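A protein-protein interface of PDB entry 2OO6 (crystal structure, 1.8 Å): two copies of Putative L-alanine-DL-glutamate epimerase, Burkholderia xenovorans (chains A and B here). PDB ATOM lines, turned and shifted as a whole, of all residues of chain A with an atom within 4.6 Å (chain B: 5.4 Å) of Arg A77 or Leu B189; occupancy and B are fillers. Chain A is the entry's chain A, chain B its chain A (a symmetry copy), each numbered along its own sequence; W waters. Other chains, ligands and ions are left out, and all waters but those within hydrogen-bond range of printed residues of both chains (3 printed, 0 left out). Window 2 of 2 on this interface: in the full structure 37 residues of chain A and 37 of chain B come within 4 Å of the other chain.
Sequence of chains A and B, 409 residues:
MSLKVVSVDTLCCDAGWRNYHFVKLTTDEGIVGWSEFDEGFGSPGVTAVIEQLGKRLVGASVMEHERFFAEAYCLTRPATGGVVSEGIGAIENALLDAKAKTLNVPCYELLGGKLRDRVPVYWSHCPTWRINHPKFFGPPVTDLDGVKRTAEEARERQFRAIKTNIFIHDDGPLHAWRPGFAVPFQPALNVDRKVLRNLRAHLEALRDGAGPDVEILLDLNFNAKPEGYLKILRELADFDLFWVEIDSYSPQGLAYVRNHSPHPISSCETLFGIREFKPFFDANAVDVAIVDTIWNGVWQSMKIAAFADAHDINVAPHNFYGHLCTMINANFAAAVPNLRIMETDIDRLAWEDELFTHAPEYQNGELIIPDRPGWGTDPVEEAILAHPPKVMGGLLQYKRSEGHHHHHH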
ATOM      1  N   TYR A  73     -20.828 -17.976  -9.933  1.00  0.00           N
ATOM      2  CA  TYR A  73     -21.262 -17.436  -8.647  1.00  0.00           C
ATOM      3  C   TYR A  73     -20.206 -16.453  -8.120  1.00  0.00           C
ATOM      4  O   TYR A  73     -20.550 -15.365  -7.657  1.00  0.00           O
ATOM      5  CB  TYR A  73     -21.476 -18.553  -7.617  1.00  0.00           C
ATOM      6  CG  TYR A  73     -21.954 -17.987  -6.277  1.00  0.00           C
ATOM      7  CD1 TYR A  73     -23.264 -17.521  -6.129  1.00  0.00           C
ATOM      8  CD2 TYR A  73     -21.098 -17.897  -5.184  1.00  0.00           C
ATOM      9  CE1 TYR A  73     -23.727 -16.969  -4.901  1.00  0.00           C
ATOM     10  CE2 TYR A  73     -21.543 -17.342  -3.949  1.00  0.00           C
ATOM     11  CZ  TYR A  73     -22.855 -16.878  -3.826  1.00  0.00           C
ATOM     12  OH  TYR A  73     -23.307 -16.351  -2.622  1.00  0.00           O
ATOM     13  N   CYS A  74     -18.924 -16.837  -8.199  1.00  0.00           N
ATOM     14  CA  CYS A  74     -17.827 -15.922  -7.827  1.00  0.00           C
ATOM     15  C   CYS A  74     -17.815 -14.638  -8.664  1.00  0.00           C
ATOM     16  O   CYS A  74     -17.732 -13.536  -8.121  1.00  0.00           O
ATOM     17  CB  CYS A  74     -16.469 -16.583  -7.988  1.00  0.00           C
ATOM     18  SG  CYS A  74     -16.141 -17.905  -6.818  1.00  0.00           S
ATOM     19  N   LEU A  75     -17.870 -14.775  -9.989  1.00  0.00           N
ATOM     20  CA  LEU A  75     -17.746 -13.605 -10.865  1.00  0.00           C
ATOM     21  C   LEU A  75     -18.892 -12.617 -10.705  1.00  0.00           C
ATOM     22  O   LEU A  75     -18.728 -11.417 -11.012  1.00  0.00           O
ATOM     23  CB  LEU A  75     -17.625 -14.016 -12.345  1.00  0.00           C
ATOM     24  CG  LEU A  75     -16.440 -14.920 -12.682  1.00  0.00           C
ATOM     25  CD1 LEU A  75     -16.622 -15.488 -14.110  1.00  0.00           C
ATOM     26  CD2 LEU A  75     -15.054 -14.216 -12.498  1.00  0.00           C
ATOM     27  N   THR A  76     -20.045 -13.103 -10.251  1.00  0.00           N
ATOM     28  CA  THR A  76     -21.218 -12.239 -10.082  1.00  0.00           C
ATOM     29  C   THR A  76     -21.651 -12.113  -8.606  1.00  0.00           C
ATOM     30  O   THR A  76     -22.755 -11.644  -8.334  1.00  0.00           O
ATOM     31  CB  THR A  76     -22.430 -12.735 -10.928  1.00  0.00           C
ATOM     32  OG1 THR A  76     -22.781 -14.064 -10.525  1.00  0.00           O
ATOM     33  CG2 THR A  76     -22.107 -12.740 -12.430  1.00  0.00           C
ATOM     34  N   ARG A  77     -20.782 -12.526  -7.679  1.00  0.00           N
ATOM     35  CA  ARG A  77     -21.123 -12.589  -6.245  1.00  0.00           C
ATOM     36  C   ARG A  77     -21.871 -11.358  -5.708  1.00  0.00           C
ATOM     37  O   ARG A  77     -22.897 -11.521  -5.056  1.00  0.00           O
ATOM     38  CB  ARG A  77     -19.852 -12.830  -5.412  1.00  0.00           C
ATOM     39  CG  ARG A  77     -20.012 -13.968  -4.427  1.00  0.00           C
ATOM     40  CD  ARG A  77     -18.805 -14.041  -3.489  1.00  0.00           C
ATOM     41  NE  ARG A  77     -18.928 -15.245  -2.661  1.00  0.00           N
ATOM     42  CZ  ARG A  77     -18.337 -16.413  -2.907  1.00  0.00           C
ATOM     43  NH1 ARG A  77     -18.566 -17.430  -2.089  1.00  0.00           N
ATOM     44  NH2 ARG A  77     -17.504 -16.570  -3.945  1.00  0.00           N
ATOM     45  N   PRO A  78     -21.369 -10.138  -5.993  1.00  0.00           N
ATOM     46  CA  PRO A  78     -21.983  -8.920  -5.434  1.00  0.00           C
ATOM     47  C   PRO A  78     -23.444  -8.667  -5.820  1.00  0.00           C
ATOM     48  O   PRO A  78     -24.175  -8.041  -5.041  1.00  0.00           O
ATOM     49  CB  PRO A  78     -21.084  -7.802  -5.958  1.00  0.00           C
ATOM     50  CG  PRO A  78     -19.721  -8.504  -6.180  1.00  0.00           C
ATOM     51  CD  PRO A  78     -20.138  -9.824  -6.753  1.00  0.00           C
ATOM     52  N   ALA A  79     -23.853  -9.116  -7.015  1.00  0.00           N
ATOM     53  CA  ALA A  79     -25.212  -8.889  -7.493  1.00  0.00           C
ATOM     54  C   ALA A  79     -25.954 -10.208  -7.716  1.00  0.00           C
ATOM     55  O   ALA A  79     -26.801 -10.327  -8.590  1.00  0.00           O
ATOM     56  CB  ALA A  79     -25.190  -8.020  -8.782  1.00  0.00           C
ATOM     57  N   THR A  80     -25.635 -11.200  -6.891  1.00  0.00           N
ATOM     58  CA  THR A  80     -26.242 -12.512  -6.999  1.00  0.00           C
ATOM     59  C   THR A  80     -27.756 -12.484  -6.697  1.00  0.00           C
ATOM     60  O   THR A  80     -28.297 -11.508  -6.120  1.00  0.00           O
ATOM     61  CB  THR A  80     -25.499 -13.579  -6.114  1.00  0.00           C
ATOM     62  OG1 THR A  80     -25.829 -14.897  -6.575  1.00  0.00           O
ATOM     63  CG2 THR A  80     -25.908 -13.451  -4.635  1.00  0.00           C
ATOM     64  N   GLY B  42     -19.705  -7.302 -11.037  1.00  0.00           N
ATOM     65  CA  GLY B  42     -20.554  -8.506 -11.052  1.00  0.00           C
ATOM     66  C   GLY B  42     -21.989  -8.297 -11.509  1.00  0.00           C
ATOM     67  O   GLY B  42     -22.866  -9.123 -11.180  1.00  0.00           O
ATOM     68  N   PRO B 179      -9.998 -14.702  -4.121  1.00  0.00           N
ATOM     69  CA  PRO B 179     -10.649 -15.960  -4.506  1.00  0.00           C
ATOM     70  C   PRO B 179     -12.188 -15.850  -4.457  1.00  0.00           C
ATOM     71  O   PRO B 179     -12.899 -16.580  -5.192  1.00  0.00           O
ATOM     72  CB  PRO B 179     -10.146 -16.946  -3.463  1.00  0.00           C
ATOM     73  CG  PRO B 179      -9.768 -16.094  -2.247  1.00  0.00           C
ATOM     74  CD  PRO B 179      -9.245 -14.817  -2.854  1.00  0.00           C
ATOM     75  N   GLY B 180     -12.710 -14.931  -3.637  1.00  0.00           N
ATOM     76  CA  GLY B 180     -14.189 -14.672  -3.624  1.00  0.00           C
ATOM     77  C   GLY B 180     -14.699 -14.262  -5.007  1.00  0.00           C
ATOM     78  O   GLY B 180     -15.865 -14.509  -5.359  1.00  0.00           O
ATOM     79  N   PHE B 181     -13.819 -13.657  -5.809  1.00  0.00           N
ATOM     80  CA  PHE B 181     -14.154 -13.303  -7.192  1.00  0.00           C
ATOM     81  C   PHE B 181     -13.389 -14.142  -8.235  1.00  0.00           C
ATOM     82  O   PHE B 181     -13.190 -13.704  -9.392  1.00  0.00           O
ATOM     83  CB  PHE B 181     -13.917 -11.812  -7.440  1.00  0.00           C
ATOM     84  CG  PHE B 181     -14.640 -10.907  -6.486  1.00  0.00           C
ATOM     85  CD1 PHE B 181     -15.950 -11.183  -6.078  1.00  0.00           C
ATOM     86  CD2 PHE B 181     -14.030  -9.723  -6.039  1.00  0.00           C
ATOM     87  CE1 PHE B 181     -16.643 -10.279  -5.231  1.00  0.00           C
ATOM     88  CE2 PHE B 181     -14.712  -8.836  -5.179  1.00  0.00           C
ATOM     89  CZ  PHE B 181     -16.005  -9.126  -4.771  1.00  0.00           C
ATOM     90  N   GLN B 186     -10.478 -20.715  -6.353  1.00  0.00           N
ATOM     91  CA  GLN B 186     -10.288 -21.624  -5.217  1.00  0.00           C
ATOM     92  C   GLN B 186     -11.570 -21.423  -4.415  1.00  0.00           C
ATOM     93  O   GLN B 186     -11.592 -20.654  -3.448  1.00  0.00           O
ATOM     94  CB  GLN B 186      -9.036 -21.259  -4.390  1.00  0.00           C
ATOM     95  CG  GLN B 186      -7.691 -21.373  -5.141  1.00  0.00           C
ATOM     96  CD  GLN B 186      -6.499 -20.910  -4.289  1.00  0.00           C
ATOM     97  OE1 GLN B 186      -6.634 -20.673  -3.073  1.00  0.00           O
ATOM     98  NE2 GLN B 186      -5.335 -20.776  -4.919  1.00  0.00           N
ATOM     99  N   PRO B 187     -12.670 -22.059  -4.864  1.00  0.00           N
ATOM    100  CA  PRO B 187     -13.986 -21.648  -4.388  1.00  0.00           C
ATOM    101  C   PRO B 187     -14.306 -21.969  -2.916  1.00  0.00           C
ATOM    102  O   PRO B 187     -15.264 -21.409  -2.373  1.00  0.00           O
ATOM    103  CB  PRO B 187     -14.942 -22.373  -5.338  1.00  0.00           C
ATOM    104  CG  PRO B 187     -14.225 -23.636  -5.688  1.00  0.00           C
ATOM    105  CD  PRO B 187     -12.768 -23.165  -5.843  1.00  0.00           C
ATOM    106  N   ALA B 188     -13.502 -22.823  -2.266  1.00  0.00           N
ATOM    107  CA  ALA B 188     -13.657 -23.026  -0.825  1.00  0.00           C
ATOM    108  C   ALA B 188     -13.305 -21.777  -0.023  1.00  0.00           C
ATOM    109  O   ALA B 188     -13.796 -21.619   1.111  1.00  0.00           O
ATOM    110  CB  ALA B 188     -12.832 -24.216  -0.355  1.00  0.00           C
ATOM    111  N   LEU B 189     -12.500 -20.875  -0.613  1.00  0.00           N
ATOM    112  CA  LEU B 189     -12.064 -19.631   0.060  1.00  0.00           C
ATOM    113  C   LEU B 189     -11.295 -19.897   1.379  1.00  0.00           C
ATOM    114  O   LEU B 189     -11.438 -19.155   2.340  1.00  0.00           O
ATOM    115  CB  LEU B 189     -13.265 -18.683   0.317  1.00  0.00           C
ATOM    116  CG  LEU B 189     -14.269 -18.481  -0.832  1.00  0.00           C
ATOM    117  CD1 LEU B 189     -15.387 -17.450  -0.410  1.00  0.00           C
ATOM    118  CD2 LEU B 189     -13.537 -18.032  -2.109  1.00  0.00           C
ATOM    119  N   ASN B 190     -10.506 -20.979   1.432  1.00  0.00           N
ATOM    120  CA  ASN B 190      -9.755 -21.260   2.644  1.00  0.00           C
ATOM    121  C   ASN B 190      -8.652 -20.207   2.810  1.00  0.00           C
ATOM    122  O   ASN B 190      -8.155 -19.652   1.814  1.00  0.00           O
ATOM    123  CB  ASN B 190      -9.142 -22.675   2.622  1.00  0.00           C
ATOM    124  CG  ASN B 190     -10.184 -23.758   2.645  1.00  0.00           C
ATOM    125  OD1 ASN B 190     -11.101 -23.745   3.471  1.00  0.00           O
ATOM    126  ND2 ASN B 190     -10.044 -24.720   1.736  1.00  0.00           N
ATOM    127  N   VAL B 191      -8.332 -19.916   4.068  1.00  0.00           N
ATOM    128  CA  VAL B 191      -7.240 -19.019   4.440  1.00  0.00           C
ATOM    129  C   VAL B 191      -6.103 -19.850   5.062  1.00  0.00           C
ATOM    130  O   VAL B 191      -6.312 -20.598   6.003  1.00  0.00           O
ATOM    131  CB  VAL B 191      -7.745 -17.937   5.436  1.00  0.00           C
ATOM    132  CG1 VAL B 191      -6.592 -17.039   5.931  1.00  0.00           C
ATOM    133  CG2 VAL B 191      -8.908 -17.122   4.827  1.00  0.00           C
ATOM    134  N   PHE B 222     -15.454 -10.647  -0.209  1.00  0.00           N
ATOM    135  CA  PHE B 222     -16.077 -11.950  -0.022  1.00  0.00           C
ATOM    136  C   PHE B 222     -14.979 -13.053  -0.028  1.00  0.00           C
ATOM    137  O   PHE B 222     -15.239 -14.170  -0.447  1.00  0.00           O
ATOM    138  CB  PHE B 222     -17.062 -12.274  -1.159  1.00  0.00           C
ATOM    139  CG  PHE B 222     -18.364 -11.477  -1.153  1.00  0.00           C
ATOM    140  CD1 PHE B 222     -19.510 -11.977  -0.518  1.00  0.00           C
ATOM    141  CD2 PHE B 222     -18.466 -10.276  -1.882  1.00  0.00           C
ATOM    142  CE1 PHE B 222     -20.720 -11.247  -0.545  1.00  0.00           C
ATOM    143  CE2 PHE B 222     -19.688  -9.568  -1.932  1.00  0.00           C
ATOM    144  CZ  PHE B 222     -20.792 -10.046  -1.286  1.00  0.00           C
ATOM    145  N   ASN B 223     -13.761 -12.735   0.428  1.00  0.00           N
ATOM    146  CA  ASN B 223     -12.604 -13.624   0.195  1.00  0.00           C
ATOM    147  C   ASN B 223     -12.343 -14.740   1.196  1.00  0.00           C
ATOM    148  O   ASN B 223     -11.314 -15.431   1.094  1.00  0.00           O
ATOM    149  CB  ASN B 223     -11.355 -12.769  -0.029  1.00  0.00           C
ATOM    150  CG  ASN B 223     -11.474 -11.970  -1.303  1.00  0.00           C
ATOM    151  OD1 ASN B 223     -11.871 -12.518  -2.346  1.00  0.00           O
ATOM    152  ND2 ASN B 223     -11.191 -10.671  -1.232  1.00  0.00           N
ATOM    153  N   ALA B 224     -13.271 -14.948   2.136  1.00  0.00           N
ATOM    154  CA  ALA B 224     -13.192 -16.107   3.060  1.00  0.00           C
ATOM    155  C   ALA B 224     -14.575 -16.613   3.508  1.00  0.00           C
ATOM    156  O   ALA B 224     -15.607 -16.051   3.109  1.00  0.00           O
ATOM    157  CB  ALA B 224     -12.336 -15.755   4.307  1.00  0.00           C
ATOM    158  N   LYS B 225     -14.587 -17.678   4.319  1.00  0.00           N
ATOM    159  CA  LYS B 225     -15.775 -18.079   5.062  1.00  0.00           C
ATOM    160  C   LYS B 225     -15.553 -17.622   6.522  1.00  0.00           C
ATOM    161  O   LYS B 225     -14.403 -17.333   6.896  1.00  0.00           O
ATOM    162  CB  LYS B 225     -15.946 -19.613   5.021  1.00  0.00           C
ATOM    163  CG  LYS B 225     -15.803 -20.273   3.606  1.00  0.00           C
ATOM    164  CD  LYS B 225     -16.876 -19.760   2.645  1.00  0.00           C
ATOM    165  CE  LYS B 225     -16.873 -20.461   1.237  1.00  0.00           C
ATOM    166  NZ  LYS B 225     -17.317 -21.878   1.267  1.00  0.00           N
ATOM    167  N   TYR B 249     -23.384 -13.094   2.965  1.00  0.00           N
ATOM    168  CA  TYR B 249     -24.817 -13.351   2.902  1.00  0.00           C
ATOM    169  C   TYR B 249     -25.320 -14.247   4.043  1.00  0.00           C
ATOM    170  O   TYR B 249     -26.437 -14.778   3.976  1.00  0.00           O
ATOM    171  CB  TYR B 249     -25.215 -13.909   1.547  1.00  0.00           C
ATOM    172  CG  TYR B 249     -24.819 -12.997   0.383  1.00  0.00           C
ATOM    173  CD1 TYR B 249     -25.038 -11.609   0.453  1.00  0.00           C
ATOM    174  CD2 TYR B 249     -24.225 -13.526  -0.784  1.00  0.00           C
ATOM    175  CE1 TYR B 249     -24.686 -10.764  -0.614  1.00  0.00           C
ATOM    176  CE2 TYR B 249     -23.861 -12.670  -1.875  1.00  0.00           C
ATOM    177  CZ  TYR B 249     -24.117 -11.297  -1.768  1.00  0.00           C
ATOM    178  OH  TYR B 249     -23.786 -10.437  -2.792  1.00  0.00           O
HETATM  179  O   HOH W   1     -26.035  -8.602  -3.059  1.00  0.00           O
HETATM  180  O   HOH W   2     -16.890 -19.516  -3.702  1.00  0.00           O
HETATM  181  O   HOH W   3     -12.939 -19.002  -6.304  1.00  0.00           O
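Water W3 lies within hydrogen-bond range of the backbone carbonyl oxygen of Pro B179, the backbone NH of Gln B186 and the side-chain sulfur of Cys A74.
Water W1 bridges the backbone carbonyl oxygen of Pro A78 (2.8 Å) and the side-chain hydroxyl of Tyr B249 (2.9 Å).
Water W2 lies within hydrogen-bond range of the backbone carbonyl oxygen (O) of Pro B187 (2.8 Å), the guanidinium group (NH2) of Arg A77 (3.0 Å) and the side-chain sulfur (SG) of Cys A74 (3.6 Å).
The backbone carbonyl oxygen (O) of Gly B180 lies close to the side-chain sulfur (SG) of Cys A74, at 3.7 Å.
O of Gly B180 sits at hydrogen-bond distance from NH2 of Arg A77 (3.0 Å).
OH of Tyr B249 lies within hydrogen-bond range of O of Arg A77.
OH of Tyr B249 lies within hydrogen-bond range of O of Pro A78 (3.3 Å).
CD2 of Tyr B249 touches OH of Tyr A73, 3.5 Å away.
Cys A74 touches Pro B179.
O of Cys A74 touches CD1 of Phe B181, at 3.6 Å.
O of Leu A75 touches CA of Gly B42 (3.4 Å).
Leu A75 touches Phe B181.
CD1 of Leu B189 touches NH1 of Arg A77, at 3.6 Å.
CD of Arg A77 touches CB of Phe B222, 3.4 Å away.
CE1 of Phe B181 touches CG of Pro A78, 3.7 Å away.
O of Gly B42 touches CB of Ala A79, 3.5 Å away.
CE2 of Tyr B249 touches CG2 of Thr A80, at 3.5 Å.
Of chain B, only Gly B180, Leu B189, Phe B222 and Tyr B249 come within 4 Å of Arg A77.
Leu B189 touches one residue of chain A.
Of the printed residues of chain B, Leu A75 touches Gly B42 (3.4 Å) and Phe B181 (3.7 Å).
Of the printed residues of chain A, Pro B179 touches Cys A74.
Printed residues of chain B within 4 Å of Pro A78: Phe B181 and Tyr B249.
Of the printed residues of chain A, Phe B181 touches Cys A74 (3.6 Å), Leu A75 (3.7 Å) and Pro A78 (3.7 Å).
Pro B187 touches none of the printed residues of chain A.
The nearest residue of chain B that does not touch Arg A77 is Phe B181 (4.1 Å).
The nearest printed residue of chain A that does not touch Leu B189 is Cys A74 (5.4 Å).
Hydrophobic or aromatic side chains of chain B that line the printed part of chain A: Phe B181, Leu B189, Phe B222 and Tyr B249.
Printed residues of chain A that touch a printed residue of chain B: Tyr A73, Cys A74, Leu A75, Thr A76, Arg A77, Pro A78, Ala A79 and Thr A80.
Among the printed residues, 15 pairs touch across the chains.
Among the printed residues, no Asp or Glu carboxylate lies within 4 Å of a Lys or Arg side-chain nitrogen of the other chain.
The side-chain amide oxygen (OD1) of Asn B223 sits at hydrogen-bond distance from the backbone NH (N) of Gly B180.
The side-chain sulfur of Cys A74 is in hydrogen-bond range of the guanidinium group of Arg A77.
No position is printed for both chains.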
